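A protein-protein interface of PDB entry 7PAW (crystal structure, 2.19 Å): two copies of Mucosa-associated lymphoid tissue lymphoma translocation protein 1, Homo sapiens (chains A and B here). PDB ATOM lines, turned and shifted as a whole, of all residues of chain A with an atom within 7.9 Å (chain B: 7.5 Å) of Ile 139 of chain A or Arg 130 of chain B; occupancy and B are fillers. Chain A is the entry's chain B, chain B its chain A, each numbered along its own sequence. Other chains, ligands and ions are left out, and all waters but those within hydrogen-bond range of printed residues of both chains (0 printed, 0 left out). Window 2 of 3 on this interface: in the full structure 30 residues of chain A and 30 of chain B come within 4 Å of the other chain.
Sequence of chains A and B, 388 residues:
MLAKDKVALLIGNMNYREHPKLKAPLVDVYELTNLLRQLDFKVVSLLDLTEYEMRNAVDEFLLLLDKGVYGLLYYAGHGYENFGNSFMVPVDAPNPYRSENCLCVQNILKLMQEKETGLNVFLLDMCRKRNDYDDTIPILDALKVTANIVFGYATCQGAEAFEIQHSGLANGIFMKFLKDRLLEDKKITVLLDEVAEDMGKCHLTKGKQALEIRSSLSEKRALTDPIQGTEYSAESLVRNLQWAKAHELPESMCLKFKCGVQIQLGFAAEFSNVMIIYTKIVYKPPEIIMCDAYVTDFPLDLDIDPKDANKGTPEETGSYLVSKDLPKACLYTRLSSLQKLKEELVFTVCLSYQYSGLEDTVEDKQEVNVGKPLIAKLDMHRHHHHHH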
ATOM      1  N   PHE A  83     -14.352  -7.913 -26.699  1.00  0.00           N
ATOM      2  CA  PHE A  83     -13.242  -8.108 -25.762  1.00  0.00           C
ATOM      3  C   PHE A  83     -13.630  -8.837 -24.455  1.00  0.00           C
ATOM      4  O   PHE A  83     -13.352  -8.353 -23.344  1.00  0.00           O
ATOM      5  CB  PHE A  83     -12.563  -6.749 -25.496  1.00  0.00           C
ATOM      6  CG  PHE A  83     -12.044  -6.129 -26.768  1.00  0.00           C
ATOM      7  CD1 PHE A  83     -10.825  -6.523 -27.303  1.00  0.00           C
ATOM      8  CD2 PHE A  83     -12.795  -5.184 -27.458  1.00  0.00           C
ATOM      9  CE1 PHE A  83     -10.347  -5.951 -28.494  1.00  0.00           C
ATOM     10  CE2 PHE A  83     -12.336  -4.637 -28.661  1.00  0.00           C
ATOM     11  CZ  PHE A  83     -11.113  -5.021 -29.173  1.00  0.00           C
ATOM     12  N   ASN A  85     -16.584  -9.307 -23.188  1.00  0.00           N
ATOM     13  CA  ASN A  85     -17.901  -8.845 -22.733  1.00  0.00           C
ATOM     14  C   ASN A  85     -19.017  -9.071 -23.745  1.00  0.00           C
ATOM     15  O   ASN A  85     -18.875  -8.671 -24.909  1.00  0.00           O
ATOM     16  CB  ASN A  85     -17.839  -7.355 -22.337  1.00  0.00           C
ATOM     17  CG  ASN A  85     -16.818  -7.025 -21.278  1.00  0.00           C
ATOM     18  OD1 ASN A  85     -15.930  -6.203 -21.481  1.00  0.00           O
ATOM     19  ND2 ASN A  85     -16.915  -7.649 -20.125  1.00  0.00           N
ATOM     20  N   ASN A 107     -22.116  -7.507 -16.111  1.00  0.00           N
ATOM     21  CA  ASN A 107     -22.660  -6.592 -15.110  1.00  0.00           C
ATOM     22  C   ASN A 107     -23.706  -7.312 -14.288  1.00  0.00           C
ATOM     23  O   ASN A 107     -23.605  -7.313 -13.064  1.00  0.00           O
ATOM     24  CB  ASN A 107     -23.296  -5.365 -15.775  1.00  0.00           C
ATOM     25  CG  ASN A 107     -22.387  -4.181 -15.892  1.00  0.00           C
ATOM     26  OD1 ASN A 107     -22.052  -3.528 -14.902  1.00  0.00           O
ATOM     27  ND2 ASN A 107     -21.992  -3.865 -17.107  1.00  0.00           N
ATOM     28  N   LYS A 110     -22.318  -9.784 -11.617  1.00  0.00           N
ATOM     29  CA  LYS A 110     -21.862  -9.115 -10.383  1.00  0.00           C
ATOM     30  C   LYS A 110     -22.982  -8.851  -9.352  1.00  0.00           C
ATOM     31  O   LYS A 110     -22.739  -8.953  -8.147  1.00  0.00           O
ATOM     32  CB  LYS A 110     -21.170  -7.785 -10.718  1.00  0.00           C
ATOM     33  CG  LYS A 110     -19.741  -7.922 -11.219  1.00  0.00           C
ATOM     34  CD  LYS A 110     -19.088  -6.556 -11.470  1.00  0.00           C
ATOM     35  CE  LYS A 110     -18.448  -5.930 -10.247  1.00  0.00           C
ATOM     36  NZ  LYS A 110     -18.082  -4.510 -10.488  1.00  0.00           N
ATOM     37  N   THR A 136     -15.596   1.684 -26.798  1.00  0.00           N
ATOM     38  CA  THR A 136     -15.560   1.644 -25.337  1.00  0.00           C
ATOM     39  C   THR A 136     -15.486   0.195 -24.885  1.00  0.00           C
ATOM     40  O   THR A 136     -16.220  -0.655 -25.386  1.00  0.00           O
ATOM     41  CB  THR A 136     -16.762   2.371 -24.705  1.00  0.00           C
ATOM     42  OG1 THR A 136     -17.955   2.111 -25.453  1.00  0.00           O
ATOM     43  CG2 THR A 136     -16.532   3.859 -24.569  1.00  0.00           C
ATOM     44  N   ILE A 137     -14.559  -0.085 -23.964  1.00  0.00           N
ATOM     45  CA  ILE A 137     -14.325  -1.419 -23.417  1.00  0.00           C
ATOM     46  C   ILE A 137     -14.513  -1.348 -21.892  1.00  0.00           C
ATOM     47  O   ILE A 137     -13.641  -0.825 -21.193  1.00  0.00           O
ATOM     48  CB  ILE A 137     -12.934  -2.002 -23.846  1.00  0.00           C
ATOM     49  CG1 ILE A 137     -12.790  -2.088 -25.373  1.00  0.00           C
ATOM     50  CG2 ILE A 137     -12.697  -3.371 -23.246  1.00  0.00           C
ATOM     51  CD1 ILE A 137     -11.551  -1.457 -25.933  1.00  0.00           C
ATOM     52  N   PRO A 138     -15.642  -1.846 -21.353  1.00  0.00           N
ATOM     53  CA  PRO A 138     -15.824  -1.825 -19.892  1.00  0.00           C
ATOM     54  C   PRO A 138     -14.849  -2.756 -19.168  1.00  0.00           C
ATOM     55  O   PRO A 138     -14.553  -3.850 -19.655  1.00  0.00           O
ATOM     56  CB  PRO A 138     -17.278  -2.316 -19.706  1.00  0.00           C
ATOM     57  CG  PRO A 138     -17.909  -2.230 -21.061  1.00  0.00           C
ATOM     58  CD  PRO A 138     -16.796  -2.488 -22.017  1.00  0.00           C
ATOM     59  N   ILE A 139     -14.338  -2.304 -18.016  1.00  0.00           N
ATOM     60  CA  ILE A 139     -13.462  -3.083 -17.137  1.00  0.00           C
ATOM     61  C   ILE A 139     -14.185  -3.163 -15.784  1.00  0.00           C
ATOM     62  O   ILE A 139     -14.326  -2.154 -15.088  1.00  0.00           O
ATOM     63  CB  ILE A 139     -11.987  -2.564 -17.057  1.00  0.00           C
ATOM     64  CG1 ILE A 139     -11.293  -2.639 -18.446  1.00  0.00           C
ATOM     65  CG2 ILE A 139     -11.192  -3.352 -15.995  1.00  0.00           C
ATOM     66  CD1 ILE A 139      -9.946  -2.015 -18.536  1.00  0.00           C
ATOM     67  N   LEU A 140     -14.697  -4.358 -15.463  1.00  0.00           N
ATOM     68  CA  LEU A 140     -15.464  -4.640 -14.250  1.00  0.00           C
ATOM     69  C   LEU A 140     -14.573  -5.180 -13.140  1.00  0.00           C
ATOM     70  O   LEU A 140     -13.598  -5.880 -13.424  1.00  0.00           O
ATOM     71  CB  LEU A 140     -16.586  -5.652 -14.557  1.00  0.00           C
ATOM     72  CG  LEU A 140     -17.637  -5.193 -15.563  1.00  0.00           C
ATOM     73  CD1 LEU A 140     -17.416  -5.828 -16.922  1.00  0.00           C
ATOM     74  CD2 LEU A 140     -19.018  -5.466 -15.059  1.00  0.00           C
ATOM     75  N   ASP A 141     -14.929  -4.868 -11.872  1.00  0.00           N
ATOM     76  CA  ASP A 141     -14.222  -5.330 -10.670  1.00  0.00           C
ATOM     77  C   ASP A 141     -14.261  -6.851 -10.563  1.00  0.00           C
ATOM     78  O   ASP A 141     -15.257  -7.473 -10.942  1.00  0.00           O
ATOM     79  CB  ASP A 141     -14.801  -4.689  -9.399  1.00  0.00           C
ATOM     80  CG  ASP A 141     -14.545  -3.197  -9.244  1.00  0.00           C
ATOM     81  OD1 ASP A 141     -15.069  -2.604  -8.275  1.00  0.00           O
ATOM     82  OD2 ASP A 141     -13.812  -2.620 -10.089  1.00  0.00           O
ATOM     83  N   ALA A 142     -13.145  -7.434 -10.078  1.00  0.00           N
ATOM     84  CA  ALA A 142     -12.896  -8.869  -9.906  1.00  0.00           C
ATOM     85  C   ALA A 142     -14.157  -9.704  -9.665  1.00  0.00           C
ATOM     86  O   ALA A 142     -14.910  -9.431  -8.723  1.00  0.00           O
ATOM     87  CB  ALA A 142     -11.879  -9.095  -8.790  1.00  0.00           C
ATOM     88  N   GLY B  79       1.088 -15.399 -14.680  1.00  0.00           N
ATOM     89  CA  GLY B  79       0.177 -15.140 -15.775  1.00  0.00           C
ATOM     90  C   GLY B  79      -0.779 -14.008 -15.473  1.00  0.00           C
ATOM     91  O   GLY B  79      -0.858 -13.547 -14.340  1.00  0.00           O
ATOM     92  N   TYR B  80      -1.503 -13.565 -16.496  1.00  0.00           N
ATOM     93  CA  TYR B  80      -2.528 -12.538 -16.444  1.00  0.00           C
ATOM     94  C   TYR B  80      -3.591 -12.732 -17.523  1.00  0.00           C
ATOM     95  O   TYR B  80      -3.404 -13.491 -18.488  1.00  0.00           O
ATOM     96  CB  TYR B  80      -1.941 -11.113 -16.463  1.00  0.00           C
ATOM     97  CG  TYR B  80      -1.407 -10.646 -17.799  1.00  0.00           C
ATOM     98  CD1 TYR B  80      -0.066 -10.821 -18.135  1.00  0.00           C
ATOM     99  CD2 TYR B  80      -2.224  -9.967 -18.700  1.00  0.00           C
ATOM    100  CE1 TYR B  80       0.452 -10.310 -19.325  1.00  0.00           C
ATOM    101  CE2 TYR B  80      -1.717  -9.445 -19.887  1.00  0.00           C
ATOM    102  CZ  TYR B  80      -0.380  -9.630 -20.203  1.00  0.00           C
ATOM    103  OH  TYR B  80       0.120  -9.108 -21.373  1.00  0.00           O
ATOM    104  N   GLU B  81      -4.707 -12.033 -17.348  1.00  0.00           N
ATOM    105  CA  GLU B  81      -5.821 -12.088 -18.266  1.00  0.00           C
ATOM    106  C   GLU B  81      -6.370 -10.712 -18.583  1.00  0.00           C
ATOM    107  O   GLU B  81      -6.907 -10.038 -17.702  1.00  0.00           O
ATOM    108  CB  GLU B  81      -6.914 -13.008 -17.724  1.00  0.00           C
ATOM    109  CG  GLU B  81      -7.872 -13.485 -18.805  1.00  0.00           C
ATOM    110  CD  GLU B  81      -8.696 -14.668 -18.356  1.00  0.00           C
ATOM    111  OE1 GLU B  81      -8.119 -15.740 -18.049  1.00  0.00           O
ATOM    112  OE2 GLU B  81      -9.931 -14.507 -18.293  1.00  0.00           O
ATOM    113  N   ASN B  82      -6.279 -10.328 -19.869  1.00  0.00           N
ATOM    114  CA  ASN B  82      -6.742  -9.040 -20.375  1.00  0.00           C
ATOM    115  C   ASN B  82      -7.611  -9.234 -21.564  1.00  0.00           C
ATOM    116  O   ASN B  82      -7.218  -9.918 -22.519  1.00  0.00           O
ATOM    117  CB  ASN B  82      -5.560  -8.121 -20.759  1.00  0.00           C
ATOM    118  CG  ASN B  82      -4.900  -7.389 -19.615  1.00  0.00           C
ATOM    119  OD1 ASN B  82      -4.629  -7.947 -18.550  1.00  0.00           O
ATOM    120  ND2 ASN B  82      -4.586  -6.126 -19.836  1.00  0.00           N
ATOM    121  N   PHE B  83      -8.803  -8.621 -21.514  1.00  0.00           N
ATOM    122  CA  PHE B  83      -9.802  -8.610 -22.586  1.00  0.00           C
ATOM    123  C   PHE B  83     -10.130 -10.000 -23.136  1.00  0.00           C
ATOM    124  O   PHE B  83     -10.268 -10.172 -24.350  1.00  0.00           O
ATOM    125  CB  PHE B  83      -9.379  -7.635 -23.699  1.00  0.00           C
ATOM    126  CG  PHE B  83      -8.946  -6.295 -23.149  1.00  0.00           C
ATOM    127  CD1 PHE B  83      -9.875  -5.419 -22.592  1.00  0.00           C
ATOM    128  CD2 PHE B  83      -7.605  -5.927 -23.148  1.00  0.00           C
ATOM    129  CE1 PHE B  83      -9.473  -4.181 -22.069  1.00  0.00           C
ATOM    130  CE2 PHE B  83      -7.203  -4.695 -22.621  1.00  0.00           C
ATOM    131  CZ  PHE B  83      -8.137  -3.826 -22.090  1.00  0.00           C
ATOM    132  N   TYR B  97       5.819  -5.719 -17.356  1.00  0.00           N
ATOM    133  CA  TYR B  97       5.729  -6.406 -18.647  1.00  0.00           C
ATOM    134  C   TYR B  97       4.436  -6.067 -19.400  1.00  0.00           C
ATOM    135  O   TYR B  97       3.405  -5.748 -18.794  1.00  0.00           O
ATOM    136  CB  TYR B  97       5.859  -7.931 -18.499  1.00  0.00           C
ATOM    137  CG  TYR B  97       4.965  -8.548 -17.443  1.00  0.00           C
ATOM    138  CD1 TYR B  97       3.648  -8.899 -17.732  1.00  0.00           C
ATOM    139  CD2 TYR B  97       5.458  -8.858 -16.183  1.00  0.00           C
ATOM    140  CE1 TYR B  97       2.824  -9.469 -16.763  1.00  0.00           C
ATOM    141  CE2 TYR B  97       4.654  -9.467 -15.221  1.00  0.00           C
ATOM    142  CZ  TYR B  97       3.340  -9.781 -15.517  1.00  0.00           C
ATOM    143  OH  TYR B  97       2.564 -10.377 -14.554  1.00  0.00           O
ATOM    144  N   CYS B 127      -2.577 -17.213 -12.211  1.00  0.00           N
ATOM    145  CA  CYS B 127      -3.522 -16.215 -11.744  1.00  0.00           C
ATOM    146  C   CYS B 127      -4.175 -15.538 -12.921  1.00  0.00           C
ATOM    147  O   CYS B 127      -3.608 -15.500 -14.019  1.00  0.00           O
ATOM    148  CB  CYS B 127      -2.855 -15.230 -10.796  1.00  0.00           C
ATOM    149  SG  CYS B 127      -2.288 -15.995  -9.263  1.00  0.00           S
ATOM    150  N   ARG B 128      -5.407 -15.103 -12.729  1.00  0.00           N
ATOM    151  CA  ARG B 128      -6.185 -14.535 -13.823  1.00  0.00           C
ATOM    152  C   ARG B 128      -6.590 -13.099 -13.630  1.00  0.00           C
ATOM    153  O   ARG B 128      -7.602 -12.671 -14.180  1.00  0.00           O
ATOM    154  CB  ARG B 128      -7.408 -15.403 -14.091  1.00  0.00           C
ATOM    155  CG  ARG B 128      -7.070 -16.788 -14.548  1.00  0.00           C
ATOM    156  CD  ARG B 128      -8.316 -17.591 -14.667  1.00  0.00           C
ATOM    157  NE  ARG B 128      -9.157 -17.129 -15.774  1.00  0.00           N
ATOM    158  CZ  ARG B 128     -10.439 -17.441 -15.901  1.00  0.00           C
ATOM    159  NH1 ARG B 128     -11.032 -18.211 -15.001  1.00  0.00           N
ATOM    160  NH2 ARG B 128     -11.139 -16.984 -16.928  1.00  0.00           N
ATOM    161  N   LYS B 129      -5.793 -12.336 -12.905  1.00  0.00           N
ATOM    162  CA  LYS B 129      -6.055 -10.908 -12.736  1.00  0.00           C
ATOM    163  C   LYS B 129      -5.500 -10.175 -13.976  1.00  0.00           C
ATOM    164  O   LYS B 129      -4.681 -10.729 -14.704  1.00  0.00           O
ATOM    165  CB  LYS B 129      -5.395 -10.389 -11.441  1.00  0.00           C
ATOM    166  CG  LYS B 129      -6.119 -10.805 -10.151  1.00  0.00           C
ATOM    167  CD  LYS B 129      -5.293 -10.532  -8.877  1.00  0.00           C
ATOM    168  CE  LYS B 129      -5.331  -9.092  -8.392  1.00  0.00           C
ATOM    169  NZ  LYS B 129      -6.642  -8.718  -7.779  1.00  0.00           N
ATOM    170  N   ARG B 130      -5.943  -8.940 -14.201  1.00  0.00           N
ATOM    171  CA  ARG B 130      -5.526  -8.057 -15.297  1.00  0.00           C
ATOM    172  C   ARG B 130      -4.116  -7.512 -15.058  1.00  0.00           C
ATOM    173  O   ARG B 130      -3.686  -7.387 -13.913  1.00  0.00           O
ATOM    174  CB  ARG B 130      -6.514  -6.860 -15.386  1.00  0.00           C
ATOM    175  CG  ARG B 130      -7.188  -6.698 -16.739  1.00  0.00           C
ATOM    176  CD  ARG B 130      -7.878  -5.354 -16.928  1.00  0.00           C
ATOM    177  NE  ARG B 130      -7.487  -4.726 -18.198  1.00  0.00           N
ATOM    178  CZ  ARG B 130      -6.518  -3.817 -18.302  1.00  0.00           C
ATOM    179  NH1 ARG B 130      -5.853  -3.423 -17.231  1.00  0.00           N
ATOM    180  NH2 ARG B 130      -6.213  -3.292 -19.482  1.00  0.00           N
ATOM    181  N   ASN B 131      -3.409  -7.165 -16.145  1.00  0.00           N
ATOM    182  CA  ASN B 131      -2.100  -6.499 -16.134  1.00  0.00           C
ATOM    183  C   ASN B 131      -2.431  -5.081 -16.570  1.00  0.00           C
ATOM    184  O   ASN B 131      -2.737  -4.843 -17.743  1.00  0.00           O
ATOM    185  CB  ASN B 131      -1.118  -7.162 -17.113  1.00  0.00           C
ATOM    186  CG  ASN B 131       0.240  -6.514 -17.293  1.00  0.00           C
ATOM    187  OD1 ASN B 131       0.635  -5.565 -16.608  1.00  0.00           O
ATOM    188  ND2 ASN B 131       0.997  -7.028 -18.238  1.00  0.00           N
ATOM    189  N   ASP B 132      -2.432  -4.149 -15.604  1.00  0.00           N
ATOM    190  CA  ASP B 132      -2.782  -2.749 -15.836  1.00  0.00           C
ATOM    191  C   ASP B 132      -1.735  -1.981 -16.652  1.00  0.00           C
ATOM    192  O   ASP B 132      -1.961  -0.822 -16.990  1.00  0.00           O
ATOM    193  CB  ASP B 132      -3.101  -2.045 -14.504  1.00  0.00           C
ATOM    194  CG  ASP B 132      -4.539  -2.192 -14.004  1.00  0.00           C
ATOM    195  OD1 ASP B 132      -5.299  -3.000 -14.585  1.00  0.00           O
ATOM    196  OD2 ASP B 132      -4.902  -1.496 -13.027  1.00  0.00           O
ATOM    197  N   TYR B 133      -0.616  -2.631 -16.992  1.00  0.00           N
ATOM    198  CA  TYR B 133       0.453  -2.040 -17.796  1.00  0.00           C
ATOM    199  C   TYR B 133       0.346  -2.459 -19.263  1.00  0.00           C
ATOM    200  O   TYR B 133       1.089  -1.947 -20.102  1.00  0.00           O
ATOM    201  CB  TYR B 133       1.829  -2.380 -17.204  1.00  0.00           C
ATOM    202  CG  TYR B 133       2.009  -1.848 -15.800  1.00  0.00           C
ATOM    203  CD1 TYR B 133       2.333  -0.513 -15.574  1.00  0.00           C
ATOM    204  CD2 TYR B 133       1.835  -2.676 -14.694  1.00  0.00           C
ATOM    205  CE1 TYR B 133       2.501  -0.016 -14.279  1.00  0.00           C
ATOM    206  CE2 TYR B 133       1.991  -2.190 -13.395  1.00  0.00           C
ATOM    207  CZ  TYR B 133       2.327  -0.860 -13.192  1.00  0.00           C
ATOM    208  OH  TYR B 133       2.494  -0.377 -11.917  1.00  0.00           O
ATOM    209  N   ASP B 134      -0.592  -3.373 -19.569  1.00  0.00           N
ATOM    210  CA  ASP B 134      -0.825  -3.873 -20.919  1.00  0.00           C
ATOM    211  C   ASP B 134      -1.919  -3.054 -21.647  1.00  0.00           C
ATOM    212  O   ASP B 134      -3.124  -3.333 -21.549  1.00  0.00           O
ATOM    213  CB  ASP B 134      -1.098  -5.389 -20.909  1.00  0.00           C
ATOM    214  CG  ASP B 134      -1.138  -6.039 -22.281  1.00  0.00           C
ATOM    215  OD1 ASP B 134      -0.548  -5.472 -23.222  1.00  0.00           O
ATOM    216  OD2 ASP B 134      -1.743  -7.121 -22.407  1.00  0.00           O
ATOM    217  N   ASP B 135      -1.450  -2.017 -22.362  1.00  0.00           N
ATOM    218  CA  ASP B 135      -2.228  -1.058 -23.153  1.00  0.00           C
ATOM    219  C   ASP B 135      -2.915  -1.713 -24.353  1.00  0.00           C
ATOM    220  O   ASP B 135      -3.920  -1.189 -24.839  1.00  0.00           O
ATOM    221  CB  ASP B 135      -1.276   0.035 -23.684  1.00  0.00           C
ATOM    222  CG  ASP B 135      -1.267   1.343 -22.915  1.00  0.00           C
ATOM    223  OD1 ASP B 135      -1.289   2.410 -23.564  1.00  0.00           O
ATOM    224  OD2 ASP B 135      -1.213   1.301 -21.662  1.00  0.00           O
ATOM    225  N   THR B 136      -2.324  -2.821 -24.856  1.00  0.00           N
ATOM    226  CA  THR B 136      -2.725  -3.591 -26.037  1.00  0.00           C
ATOM    227  C   THR B 136      -4.202  -3.975 -26.040  1.00  0.00           C
ATOM    228  O   THR B 136      -4.776  -4.315 -25.007  1.00  0.00           O
ATOM    229  CB  THR B 136      -1.809  -4.824 -26.229  1.00  0.00           C
ATOM    230  OG1 THR B 136      -0.483  -4.501 -25.819  1.00  0.00           O
ATOM    231  CG2 THR B 136      -1.776  -5.329 -27.667  1.00  0.00           C
ATOM    232  N   ILE B 137      -4.801  -3.874 -27.227  1.00  0.00           N
ATOM    233  CA  ILE B 137      -6.179  -4.207 -27.542  1.00  0.00           C
ATOM    234  C   ILE B 137      -6.123  -5.369 -28.554  1.00  0.00           C
ATOM    235  O   ILE B 137      -5.543  -5.217 -29.634  1.00  0.00           O
ATOM    236  CB  ILE B 137      -6.944  -2.932 -28.012  1.00  0.00           C
ATOM    237  CG1 ILE B 137      -7.390  -2.054 -26.808  1.00  0.00           C
ATOM    238  CG2 ILE B 137      -8.101  -3.209 -28.970  1.00  0.00           C
ATOM    239  CD1 ILE B 137      -8.150  -2.755 -25.643  1.00  0.00           C
ATOM    240  N   GLN B 157     -11.989 -15.949 -13.032  1.00  0.00           N
ATOM    241  CA  GLN B 157     -11.572 -14.644 -13.557  1.00  0.00           C
ATOM    242  C   GLN B 157     -11.448 -13.604 -12.464  1.00  0.00           C
ATOM    243  O   GLN B 157     -12.357 -13.469 -11.641  1.00  0.00           O
ATOM    244  CB  GLN B 157     -12.603 -14.172 -14.574  1.00  0.00           C
ATOM    245  CG  GLN B 157     -12.031 -13.634 -15.866  1.00  0.00           C
ATOM    246  CD  GLN B 157     -13.058 -13.701 -16.974  1.00  0.00           C
ATOM    247  OE1 GLN B 157     -14.277 -13.707 -16.740  1.00  0.00           O
ATOM    248  NE2 GLN B 157     -12.586 -13.757 -18.215  1.00  0.00           N
ATOM    249  N   GLY B 158     -10.311 -12.905 -12.450  1.00  0.00           N
ATOM    250  CA  GLY B 158     -10.017 -11.850 -11.482  1.00  0.00           C
ATOM    251  C   GLY B 158      -9.615 -12.334 -10.104  1.00  0.00           C
ATOM    252  O   GLY B 158      -9.447 -11.521  -9.191  1.00  0.00           O
ATOM    253  N   ALA B 159      -9.452 -13.663  -9.953  1.00  0.00           N
ATOM    254  CA  ALA B 159      -9.048 -14.334  -8.721  1.00  0.00           C
ATOM    255  C   ALA B 159      -7.598 -14.860  -8.802  1.00  0.00           C
ATOM    256  O   ALA B 159      -7.039 -14.994  -9.902  1.00  0.00           O
ATOM    257  CB  ALA B 159     -10.011 -15.469  -8.405  1.00  0.00           C
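The backbone NH (N) of Gly 158 of chain B sits at hydrogen-bond distance from the backbone carbonyl oxygen (O) of Arg 128 of chain B (3.2 Å). The side-chain amide nitrogen (ND2) of Asn 82 of chain B sits close to the guanidinium group (NH2) of Arg 130 of chain B, at 3.3 Å. NH1 of Arg 130 of chain B is in salt-bridge range of OD1 of Asp 132 of chain B (2.7 Å).
Of the printed residues of chain B, Phe 83 of chain A touches Phe 83 (3.6 Å) and Ile 137 (3.5 Å). Printed residues of chain B within 4 Å of Ile 137 of chain A: Phe 83 (3.5 Å) and Ile 137 (3.7 Å). Ile 139 of chain A touches just one residue of chain B: Arg 130. Of the printed residues of chain A, Phe 83 of chain B touches Phe 83 (3.6 Å) and Ile 137 (3.5 Å). Arg 130 of chain B touches one residue of chain A. The nearest printed residue of chain B that does not touch Ile 137 of chain A is Arg 130 of chain B (7.4 Å).
Of the 20 printed residues of chain B, 4 touch a printed residue of chain A. Of the 11 printed residues of chain A, 4 touch a printed residue of chain B. Among the printed residues, 6 pairs touch across the chains.
Among the printed residues, pairs that only touch across the chains: Ala 142 of chain A with Gly 158 of chain B (3.5 Å), Phe 83 of chain A with Ile 137 of chain B (3.5 Å), Ile 137 of chain A with Phe 83 of chain B (3.5 Å), Phe 83 of chain A with Phe 83 of chain B (3.6 Å), Ile 137 of chain A with Ile 137 of chain B (3.7 Å) and Ile 139 of chain A with Arg 130 of chain B (3.7 Å).
Phe 83 of chain A touches its own counterpart, Phe 83 of chain B. Phe 83 of chain A touches Ile 137 of chain B, and with the chains exchanged Ile 137 of chain A touches Phe 83 of chain B. Ile 137 of chain A touches its own counterpart, Ile 137 of chain B. 3 positions are printed for both chains. Of the 6 pairs that touch across the chains among the printed residues, 4 have their exchanged pair printed and touching as well.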
